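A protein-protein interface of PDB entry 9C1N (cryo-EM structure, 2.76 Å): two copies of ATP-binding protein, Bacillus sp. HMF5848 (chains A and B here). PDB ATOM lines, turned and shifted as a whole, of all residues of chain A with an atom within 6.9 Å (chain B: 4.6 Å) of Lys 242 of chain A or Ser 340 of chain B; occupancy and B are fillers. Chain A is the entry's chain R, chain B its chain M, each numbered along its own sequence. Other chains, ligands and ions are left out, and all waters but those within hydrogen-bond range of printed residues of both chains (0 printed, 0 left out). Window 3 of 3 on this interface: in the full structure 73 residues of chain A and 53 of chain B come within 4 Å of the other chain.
The side-chain hydroxyl (OG) of Ser 219 of chain A sits close to the guanidinium group (NH1) of Arg 341 of chain B, at 2.3 Å.
The side-chain hydroxyl (OG1) of Thr 344 of chain B sits at hydrogen-bond distance from the side-chain carboxylate (OD2) of Asp 262 of chain A.
O of Arg 337 of chain B is in hydrogen-bond range of OG of Ser 340 of chain B.
O of Ser 340 of chain B lies within hydrogen-bond range of OG1 of Thr 344 of chain B (2.6 Å).
The side-chain carboxylate (OE2) of Glu 223 of chain A is in salt-bridge range of the side-chain amino group (NZ) of Lys 242 of chain A, 2.5 Å away.
The backbone carbonyl oxygen (O) of Asn 336 of chain B sits at hydrogen-bond distance from the side-chain hydroxyl (OG) of Ser 340 of chain B (3.4 Å).
OD1 of Asp 262 of chain A is in hydrogen-bond range of N of Ser 219 of chain A (2.5 Å).
Ser 340 of chain B touches Lys 242 of chain A.
Printed residues of chain B within 4 Å of Ser 219 of chain A: Arg 341 (2.3 Å).
Lys 242 of chain A touches one residue of chain B.
Arg 243 of chain A touches none of the printed residues of chain B.
Printed residues of chain B within 4 Å of Asp 262 of chain A: Thr 344.
Arg 337 of chain B touches none of the printed residues of chain A.
Of the printed residues of chain A, Ser 340 of chain B touches Lys 242.
Of the printed residues of chain A, Arg 341 of chain B touches Ser 219.
Of the printed residues of chain A, Thr 344 of chain B touches Asp 262.
The nearest printed residue of chain B that does not touch Lys 242 of chain A is Asn 336 of chain B (4.7 Å).
The nearest printed residue of chain A that does not touch Arg 341 of chain B is Glu 223 of chain A (4.3 Å).
Of the 19 printed residues of chain A, 3 touch a printed residue of chain B.
Along chain B the printed residues that touch a printed residue of chain A span positions 340 to 344.
Among the printed residues, no Asp or Glu carboxylate lies within 4 Å of a Lys or Arg side-chain nitrogen of the other chain.
No position is printed for both chains.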
ATOM      1  N   SER A 219      25.725   1.026 -14.281  1.00  0.00           N
ATOM      2  CA  SER A 219      25.320  -0.128 -15.078  1.00  0.00           C
ATOM      3  C   SER A 219      25.438  -1.428 -14.290  1.00  0.00           C
ATOM      4  O   SER A 219      24.499  -2.235 -14.258  1.00  0.00           O
ATOM      5  CB  SER A 219      26.165  -0.192 -16.351  1.00  0.00           C
ATOM      6  OG  SER A 219      27.524  -0.450 -16.048  1.00  0.00           O
ATOM      7  N   GLU A 223      22.255  -3.837 -13.238  1.00  0.00           N
ATOM      8  CA  GLU A 223      22.178  -5.189 -13.780  1.00  0.00           C
ATOM      9  C   GLU A 223      22.165  -6.231 -12.670  1.00  0.00           C
ATOM     10  O   GLU A 223      21.377  -7.183 -12.714  1.00  0.00           O
ATOM     11  CB  GLU A 223      23.342  -5.435 -14.740  1.00  0.00           C
ATOM     12  CG  GLU A 223      23.209  -4.710 -16.071  1.00  0.00           C
ATOM     13  CD  GLU A 223      24.323  -5.052 -17.040  1.00  0.00           C
ATOM     14  OE1 GLU A 223      25.082  -6.005 -16.763  1.00  0.00           O
ATOM     15  OE2 GLU A 223      24.439  -4.370 -18.080  1.00  0.00           O
ATOM     16  N   ILE A 227      18.604  -7.787 -13.245  1.00  0.00           N
ATOM     17  CA  ILE A 227      18.726  -8.874 -14.213  1.00  0.00           C
ATOM     18  C   ILE A 227      19.252 -10.145 -13.553  1.00  0.00           C
ATOM     19  O   ILE A 227      18.749 -11.245 -13.813  1.00  0.00           O
ATOM     20  CB  ILE A 227      19.617  -8.433 -15.386  1.00  0.00           C
ATOM     21  CG1 ILE A 227      18.941  -7.304 -16.163  1.00  0.00           C
ATOM     22  CG2 ILE A 227      19.910  -9.608 -16.305  1.00  0.00           C
ATOM     23  CD1 ILE A 227      19.797  -6.727 -17.260  1.00  0.00           C
ATOM     24  N   GLN A 237      18.197 -10.686 -23.175  1.00  0.00           N
ATOM     25  CA  GLN A 237      17.531 -10.187 -21.976  1.00  0.00           C
ATOM     26  C   GLN A 237      18.232  -8.971 -21.387  1.00  0.00           C
ATOM     27  O   GLN A 237      17.588  -7.952 -21.118  1.00  0.00           O
ATOM     28  CB  GLN A 237      17.441 -11.289 -20.914  1.00  0.00           C
ATOM     29  CG  GLN A 237      16.176 -12.119 -20.983  1.00  0.00           C
ATOM     30  CD  GLN A 237      15.905 -12.867 -19.693  1.00  0.00           C
ATOM     31  OE1 GLN A 237      16.660 -12.757 -18.727  1.00  0.00           O
ATOM     32  NE2 GLN A 237      14.827 -13.642 -19.675  1.00  0.00           N
ATOM     33  N   VAL A 238      19.546  -9.063 -21.174  1.00  0.00           N
ATOM     34  CA  VAL A 238      20.299  -7.932 -20.641  1.00  0.00           C
ATOM     35  C   VAL A 238      20.240  -6.756 -21.606  1.00  0.00           C
ATOM     36  O   VAL A 238      20.067  -5.602 -21.195  1.00  0.00           O
ATOM     37  CB  VAL A 238      21.750  -8.348 -20.341  1.00  0.00           C
ATOM     38  CG1 VAL A 238      22.507  -7.207 -19.678  1.00  0.00           C
ATOM     39  CG2 VAL A 238      21.775  -9.593 -19.468  1.00  0.00           C
ATOM     40  N   SER A 239      20.385  -7.030 -22.905  1.00  0.00           N
ATOM     41  CA  SER A 239      20.326  -5.964 -23.898  1.00  0.00           C
ATOM     42  C   SER A 239      18.957  -5.298 -23.919  1.00  0.00           C
ATOM     43  O   SER A 239      18.861  -4.067 -23.995  1.00  0.00           O
ATOM     44  CB  SER A 239      20.673  -6.518 -25.281  1.00  0.00           C
ATOM     45  OG  SER A 239      20.289  -5.615 -26.303  1.00  0.00           O
ATOM     46  N   GLN A 240      17.884  -6.092 -23.857  1.00  0.00           N
ATOM     47  CA  GLN A 240      16.542  -5.520 -23.885  1.00  0.00           C
ATOM     48  C   GLN A 240      16.275  -4.662 -22.655  1.00  0.00           C
ATOM     49  O   GLN A 240      15.711  -3.567 -22.765  1.00  0.00           O
ATOM     50  CB  GLN A 240      15.496  -6.629 -24.002  1.00  0.00           C
ATOM     51  CG  GLN A 240      15.315  -7.157 -25.414  1.00  0.00           C
ATOM     52  CD  GLN A 240      15.093  -6.047 -26.422  1.00  0.00           C
ATOM     53  OE1 GLN A 240      15.943  -5.785 -27.272  1.00  0.00           O
ATOM     54  NE2 GLN A 240      13.942  -5.388 -26.332  1.00  0.00           N
ATOM     55  N   PHE A 241      16.672  -5.142 -21.474  1.00  0.00           N
ATOM     56  CA  PHE A 241      16.483  -4.349 -20.263  1.00  0.00           C
ATOM     57  C   PHE A 241      17.310  -3.072 -20.309  1.00  0.00           C
ATOM     58  O   PHE A 241      16.831  -1.999 -19.922  1.00  0.00           O
ATOM     59  CB  PHE A 241      16.841  -5.171 -19.026  1.00  0.00           C
ATOM     60  CG  PHE A 241      16.633  -4.433 -17.736  1.00  0.00           C
ATOM     61  CD1 PHE A 241      15.358  -4.249 -17.228  1.00  0.00           C
ATOM     62  CD2 PHE A 241      17.709  -3.909 -17.039  1.00  0.00           C
ATOM     63  CE1 PHE A 241      15.162  -3.567 -16.045  1.00  0.00           C
ATOM     64  CE2 PHE A 241      17.517  -3.226 -15.856  1.00  0.00           C
ATOM     65  CZ  PHE A 241      16.241  -3.054 -15.360  1.00  0.00           C
ATOM     66  N   LYS A 242      18.557  -3.169 -20.776  1.00  0.00           N
ATOM     67  CA  LYS A 242      19.406  -1.988 -20.901  1.00  0.00           C
ATOM     68  C   LYS A 242      18.773  -0.962 -21.832  1.00  0.00           C
ATOM     69  O   LYS A 242      18.725   0.236 -21.521  1.00  0.00           O
ATOM     70  CB  LYS A 242      20.784  -2.405 -21.415  1.00  0.00           C
ATOM     71  CG  LYS A 242      21.849  -1.329 -21.351  1.00  0.00           C
ATOM     72  CD  LYS A 242      23.109  -1.769 -22.083  1.00  0.00           C
ATOM     73  CE  LYS A 242      23.609  -3.117 -21.581  1.00  0.00           C
ATOM     74  NZ  LYS A 242      24.035  -3.073 -20.156  1.00  0.00           N
ATOM     75  N   ARG A 243      18.270  -1.425 -22.979  1.00  0.00           N
ATOM     76  CA  ARG A 243      17.616  -0.535 -23.930  1.00  0.00           C
ATOM     77  C   ARG A 243      16.377   0.105 -23.322  1.00  0.00           C
ATOM     78  O   ARG A 243      16.137   1.302 -23.504  1.00  0.00           O
ATOM     79  CB  ARG A 243      17.253  -1.303 -25.200  1.00  0.00           C
ATOM     80  CG  ARG A 243      16.925  -0.420 -26.391  1.00  0.00           C
ATOM     81  CD  ARG A 243      16.695  -1.256 -27.640  1.00  0.00           C
ATOM     82  NE  ARG A 243      17.896  -1.363 -28.457  1.00  0.00           N
ATOM     83  CZ  ARG A 243      18.529  -2.500 -28.712  1.00  0.00           C
ATOM     84  NH1 ARG A 243      18.099  -3.653 -28.223  1.00  0.00           N
ATOM     85  NH2 ARG A 243      19.619  -2.481 -29.472  1.00  0.00           N
ATOM     86  N   ALA A 244      15.578  -0.678 -22.595  1.00  0.00           N
ATOM     87  CA  ALA A 244      14.379  -0.130 -21.971  1.00  0.00           C
ATOM     88  C   ALA A 244      14.729   0.949 -20.953  1.00  0.00           C
ATOM     89  O   ALA A 244      14.100   2.013 -20.926  1.00  0.00           O
ATOM     90  CB  ALA A 244      13.571  -1.248 -21.313  1.00  0.00           C
ATOM     91  N   VAL A 245      15.739   0.698 -20.117  1.00  0.00           N
ATOM     92  CA  VAL A 245      16.116   1.678 -19.098  1.00  0.00           C
ATOM     93  C   VAL A 245      16.638   2.955 -19.745  1.00  0.00           C
ATOM     94  O   VAL A 245      16.258   4.065 -19.351  1.00  0.00           O
ATOM     95  CB  VAL A 245      17.138   1.084 -18.113  1.00  0.00           C
ATOM     96  CG1 VAL A 245      17.422   2.076 -16.999  1.00  0.00           C
ATOM     97  CG2 VAL A 245      16.594  -0.189 -17.502  1.00  0.00           C
ATOM     98  N   VAL A 246      17.512   2.829 -20.750  1.00  0.00           N
ATOM     99  CA  VAL A 246      18.074   4.037 -21.350  1.00  0.00           C
ATOM    100  C   VAL A 246      16.999   4.803 -22.116  1.00  0.00           C
ATOM    101  O   VAL A 246      16.971   6.040 -22.103  1.00  0.00           O
ATOM    102  CB  VAL A 246      19.291   3.706 -22.239  1.00  0.00           C
ATOM    103  CG1 VAL A 246      18.924   2.751 -23.357  1.00  0.00           C
ATOM    104  CG2 VAL A 246      19.911   4.983 -22.798  1.00  0.00           C
ATOM    105  N   LEU A 247      16.083   4.088 -22.778  1.00  0.00           N
ATOM    106  CA  LEU A 247      15.003   4.750 -23.500  1.00  0.00           C
ATOM    107  C   LEU A 247      14.057   5.469 -22.548  1.00  0.00           C
ATOM    108  O   LEU A 247      13.597   6.577 -22.845  1.00  0.00           O
ATOM    109  CB  LEU A 247      14.241   3.734 -24.349  1.00  0.00           C
ATOM    110  CG  LEU A 247      14.771   3.510 -25.767  1.00  0.00           C
ATOM    111  CD1 LEU A 247      13.958   2.442 -26.481  1.00  0.00           C
ATOM    112  CD2 LEU A 247      14.768   4.812 -26.556  1.00  0.00           C
ATOM    113  N   ASN A 248      13.746   4.859 -21.401  1.00  0.00           N
ATOM    114  CA  ASN A 248      12.882   5.523 -20.430  1.00  0.00           C
ATOM    115  C   ASN A 248      13.588   6.728 -19.816  1.00  0.00           C
ATOM    116  O   ASN A 248      12.958   7.763 -19.562  1.00  0.00           O
ATOM    117  CB  ASN A 248      12.448   4.525 -19.354  1.00  0.00           C
ATOM    118  CG  ASN A 248      11.383   5.083 -18.421  1.00  0.00           C
ATOM    119  OD1 ASN A 248      10.966   6.234 -18.543  1.00  0.00           O
ATOM    120  ND2 ASN A 248      10.932   4.256 -17.486  1.00  0.00           N
ATOM    121  N   TYR A 261      23.323   4.701 -20.481  1.00  0.00           N
ATOM    122  CA  TYR A 261      22.956   3.697 -19.490  1.00  0.00           C
ATOM    123  C   TYR A 261      23.535   3.998 -18.114  1.00  0.00           C
ATOM    124  O   TYR A 261      22.988   3.535 -17.108  1.00  0.00           O
ATOM    125  CB  TYR A 261      23.411   2.316 -19.962  1.00  0.00           C
ATOM    126  CG  TYR A 261      22.854   1.172 -19.148  1.00  0.00           C
ATOM    127  CD1 TYR A 261      21.506   1.121 -18.817  1.00  0.00           C
ATOM    128  CD2 TYR A 261      23.673   0.138 -18.721  1.00  0.00           C
ATOM    129  CE1 TYR A 261      20.994   0.073 -18.075  1.00  0.00           C
ATOM    130  CE2 TYR A 261      23.170  -0.913 -17.979  1.00  0.00           C
ATOM    131  CZ  TYR A 261      21.831  -0.941 -17.659  1.00  0.00           C
ATOM    132  OH  TYR A 261      21.328  -1.986 -16.921  1.00  0.00           O
ATOM    133  N   ASP A 262      24.626   4.758 -18.046  1.00  0.00           N
ATOM    134  CA  ASP A 262      25.251   5.123 -16.783  1.00  0.00           C
ATOM    135  C   ASP A 262      24.936   6.552 -16.364  1.00  0.00           C
ATOM    136  O   ASP A 262      25.490   7.033 -15.370  1.00  0.00           O
ATOM    137  CB  ASP A 262      26.764   4.918 -16.872  1.00  0.00           C
ATOM    138  CG  ASP A 262      27.168   3.481 -16.621  1.00  0.00           C
ATOM    139  OD1 ASP A 262      26.764   2.922 -15.581  1.00  0.00           O
ATOM    140  OD2 ASP A 262      27.874   2.904 -17.473  1.00  0.00           O
ATOM    141  N   VAL A 272       9.421   0.318 -17.409  1.00  0.00           N
ATOM    142  CA  VAL A 272      10.321  -0.680 -17.980  1.00  0.00           C
ATOM    143  C   VAL A 272       9.727  -2.073 -17.825  1.00  0.00           C
ATOM    144  O   VAL A 272       9.793  -2.896 -18.745  1.00  0.00           O
ATOM    145  CB  VAL A 272      11.714  -0.576 -17.329  1.00  0.00           C
ATOM    146  CG1 VAL A 272      12.579  -1.766 -17.719  1.00  0.00           C
ATOM    147  CG2 VAL A 272      12.387   0.730 -17.722  1.00  0.00           C
ATOM    148  N   ILE A 276       8.808  -4.857 -20.720  1.00  0.00           N
ATOM    149  CA  ILE A 276       9.111  -6.285 -20.701  1.00  0.00           C
ATOM    150  C   ILE A 276       7.833  -7.104 -20.579  1.00  0.00           C
ATOM    151  O   ILE A 276       7.770  -8.242 -21.062  1.00  0.00           O
ATOM    152  CB  ILE A 276      10.110  -6.620 -19.579  1.00  0.00           C
ATOM    153  CG1 ILE A 276      11.193  -5.544 -19.484  1.00  0.00           C
ATOM    154  CG2 ILE A 276      10.739  -7.986 -19.808  1.00  0.00           C
ATOM    155  CD1 ILE A 276      12.148  -5.532 -20.661  1.00  0.00           C
ATOM    156  N   ASN B 336      27.771  -7.932 -25.041  1.00  0.00           N
ATOM    157  CA  ASN B 336      26.867  -7.010 -24.359  1.00  0.00           C
ATOM    158  C   ASN B 336      27.540  -6.356 -23.157  1.00  0.00           C
ATOM    159  O   ASN B 336      27.552  -5.124 -23.030  1.00  0.00           O
ATOM    160  CB  ASN B 336      25.594  -7.744 -23.933  1.00  0.00           C
ATOM    161  CG  ASN B 336      25.883  -9.081 -23.278  1.00  0.00           C
ATOM    162  OD1 ASN B 336      27.027  -9.536 -23.249  1.00  0.00           O
ATOM    163  ND2 ASN B 336      24.845  -9.717 -22.746  1.00  0.00           N
ATOM    164  N   ARG B 337      28.115  -7.165 -22.264  1.00  0.00           N
ATOM    165  CA  ARG B 337      28.830  -6.610 -21.119  1.00  0.00           C
ATOM    166  C   ARG B 337      30.077  -5.860 -21.567  1.00  0.00           C
ATOM    167  O   ARG B 337      30.426  -4.819 -20.994  1.00  0.00           O
ATOM    168  CB  ARG B 337      29.193  -7.721 -20.133  1.00  0.00           C
ATOM    169  CG  ARG B 337      28.053  -8.158 -19.221  1.00  0.00           C
ATOM    170  CD  ARG B 337      27.093  -9.104 -19.925  1.00  0.00           C
ATOM    171  NE  ARG B 337      27.758 -10.316 -20.386  1.00  0.00           N
ATOM    172  CZ  ARG B 337      27.721 -11.479 -19.751  1.00  0.00           C
ATOM    173  NH1 ARG B 337      27.057 -11.625 -18.616  1.00  0.00           N
ATOM    174  NH2 ARG B 337      28.367 -12.521 -20.266  1.00  0.00           N
ATOM    175  N   PHE B 338      30.762  -6.380 -22.588  1.00  0.00           N
ATOM    176  CA  PHE B 338      31.925  -5.693 -23.138  1.00  0.00           C
ATOM    177  C   PHE B 338      31.525  -4.321 -23.674  1.00  0.00           C
ATOM    178  O   PHE B 338      32.181  -3.314 -23.389  1.00  0.00           O
ATOM    179  CB  PHE B 338      32.552  -6.561 -24.236  1.00  0.00           C
ATOM    180  CG  PHE B 338      33.780  -5.969 -24.888  1.00  0.00           C
ATOM    181  CD1 PHE B 338      34.523  -4.975 -24.269  1.00  0.00           C
ATOM    182  CD2 PHE B 338      34.189  -6.421 -26.131  1.00  0.00           C
ATOM    183  CE1 PHE B 338      35.644  -4.445 -24.880  1.00  0.00           C
ATOM    184  CE2 PHE B 338      35.309  -5.894 -26.745  1.00  0.00           C
ATOM    185  CZ  PHE B 338      36.038  -4.906 -26.119  1.00  0.00           C
ATOM    186  N   LEU B 339      30.421  -4.261 -24.425  1.00  0.00           N
ATOM    187  CA  LEU B 339      29.949  -2.985 -24.954  1.00  0.00           C
ATOM    188  C   LEU B 339      29.552  -2.030 -23.836  1.00  0.00           C
ATOM    189  O   LEU B 339      29.833  -0.828 -23.909  1.00  0.00           O
ATOM    190  CB  LEU B 339      28.772  -3.212 -25.903  1.00  0.00           C
ATOM    191  CG  LEU B 339      29.112  -3.577 -27.348  1.00  0.00           C
ATOM    192  CD1 LEU B 339      27.883  -4.121 -28.059  1.00  0.00           C
ATOM    193  CD2 LEU B 339      29.672  -2.370 -28.085  1.00  0.00           C
ATOM    194  N   SER B 340      28.886  -2.544 -22.798  1.00  0.00           N
ATOM    195  CA  SER B 340      28.468  -1.687 -21.691  1.00  0.00           C
ATOM    196  C   SER B 340      29.673  -1.086 -20.975  1.00  0.00           C
ATOM    197  O   SER B 340      29.731   0.129 -20.741  1.00  0.00           O
ATOM    198  CB  SER B 340      27.602  -2.482 -20.713  1.00  0.00           C
ATOM    199  OG  SER B 340      28.340  -3.534 -20.117  1.00  0.00           O
ATOM    200  N   ARG B 341      30.653  -1.924 -20.627  1.00  0.00           N
ATOM    201  CA  ARG B 341      31.860  -1.420 -19.977  1.00  0.00           C
ATOM    202  C   ARG B 341      32.627  -0.473 -20.885  1.00  0.00           C
ATOM    203  O   ARG B 341      33.231   0.495 -20.409  1.00  0.00           O
ATOM    204  CB  ARG B 341      32.761  -2.583 -19.550  1.00  0.00           C
ATOM    205  CG  ARG B 341      32.156  -3.520 -18.516  1.00  0.00           C
ATOM    206  CD  ARG B 341      31.111  -2.818 -17.668  1.00  0.00           C
ATOM    207  NE  ARG B 341      30.385  -3.743 -16.810  1.00  0.00           N
ATOM    208  CZ  ARG B 341      29.409  -3.387 -15.988  1.00  0.00           C
ATOM    209  NH1 ARG B 341      29.035  -2.126 -15.866  1.00  0.00           N
ATOM    210  NH2 ARG B 341      28.794  -4.322 -15.271  1.00  0.00           N
ATOM    211  N   PHE B 342      32.599  -0.723 -22.193  1.00  0.00           N
ATOM    212  CA  PHE B 342      33.362   0.101 -23.115  1.00  0.00           C
ATOM    213  C   PHE B 342      32.732   1.485 -23.243  1.00  0.00           C
ATOM    214  O   PHE B 342      33.437   2.502 -23.254  1.00  0.00           O
ATOM    215  CB  PHE B 342      33.435  -0.616 -24.461  1.00  0.00           C
ATOM    216  CG  PHE B 342      34.229   0.102 -25.492  1.00  0.00           C
ATOM    217  CD1 PHE B 342      35.608   0.091 -25.429  1.00  0.00           C
ATOM    218  CD2 PHE B 342      33.619   0.775 -26.524  1.00  0.00           C
ATOM    219  CE1 PHE B 342      36.362   0.739 -26.374  1.00  0.00           C
ATOM    220  CE2 PHE B 342      34.377   1.423 -27.464  1.00  0.00           C
ATOM    221  CZ  PHE B 342      35.740   1.404 -27.391  1.00  0.00           C
ATOM    222  N   GLU B 343      31.396   1.539 -23.307  1.00  0.00           N
ATOM    223  CA  GLU B 343      30.695   2.819 -23.264  1.00  0.00           C
ATOM    224  C   GLU B 343      30.939   3.536 -21.943  1.00  0.00           C
ATOM    225  O   GLU B 343      31.128   4.759 -21.920  1.00  0.00           O
ATOM    226  CB  GLU B 343      29.195   2.611 -23.479  1.00  0.00           C
ATOM    227  CG  GLU B 343      28.460   3.861 -23.946  1.00  0.00           C
ATOM    228  CD  GLU B 343      26.956   3.666 -24.017  1.00  0.00           C
ATOM    229  OE1 GLU B 343      26.328   3.487 -22.952  1.00  0.00           O
ATOM    230  OE2 GLU B 343      26.402   3.695 -25.136  1.00  0.00           O
ATOM    231  N   THR B 344      30.931   2.796 -20.831  1.00  0.00           N
ATOM    232  CA  THR B 344      31.216   3.407 -19.535  1.00  0.00           C
ATOM    233  C   THR B 344      32.599   4.043 -19.520  1.00  0.00           C
ATOM    234  O   THR B 344      32.780   5.148 -18.993  1.00  0.00           O
ATOM    235  CB  THR B 344      31.100   2.364 -18.422  1.00  0.00           C
ATOM    236  OG1 THR B 344      29.936   1.557 -18.635  1.00  0.00           O
ATOM    237  CG2 THR B 344      31.016   3.041 -17.060  1.00  0.00           C
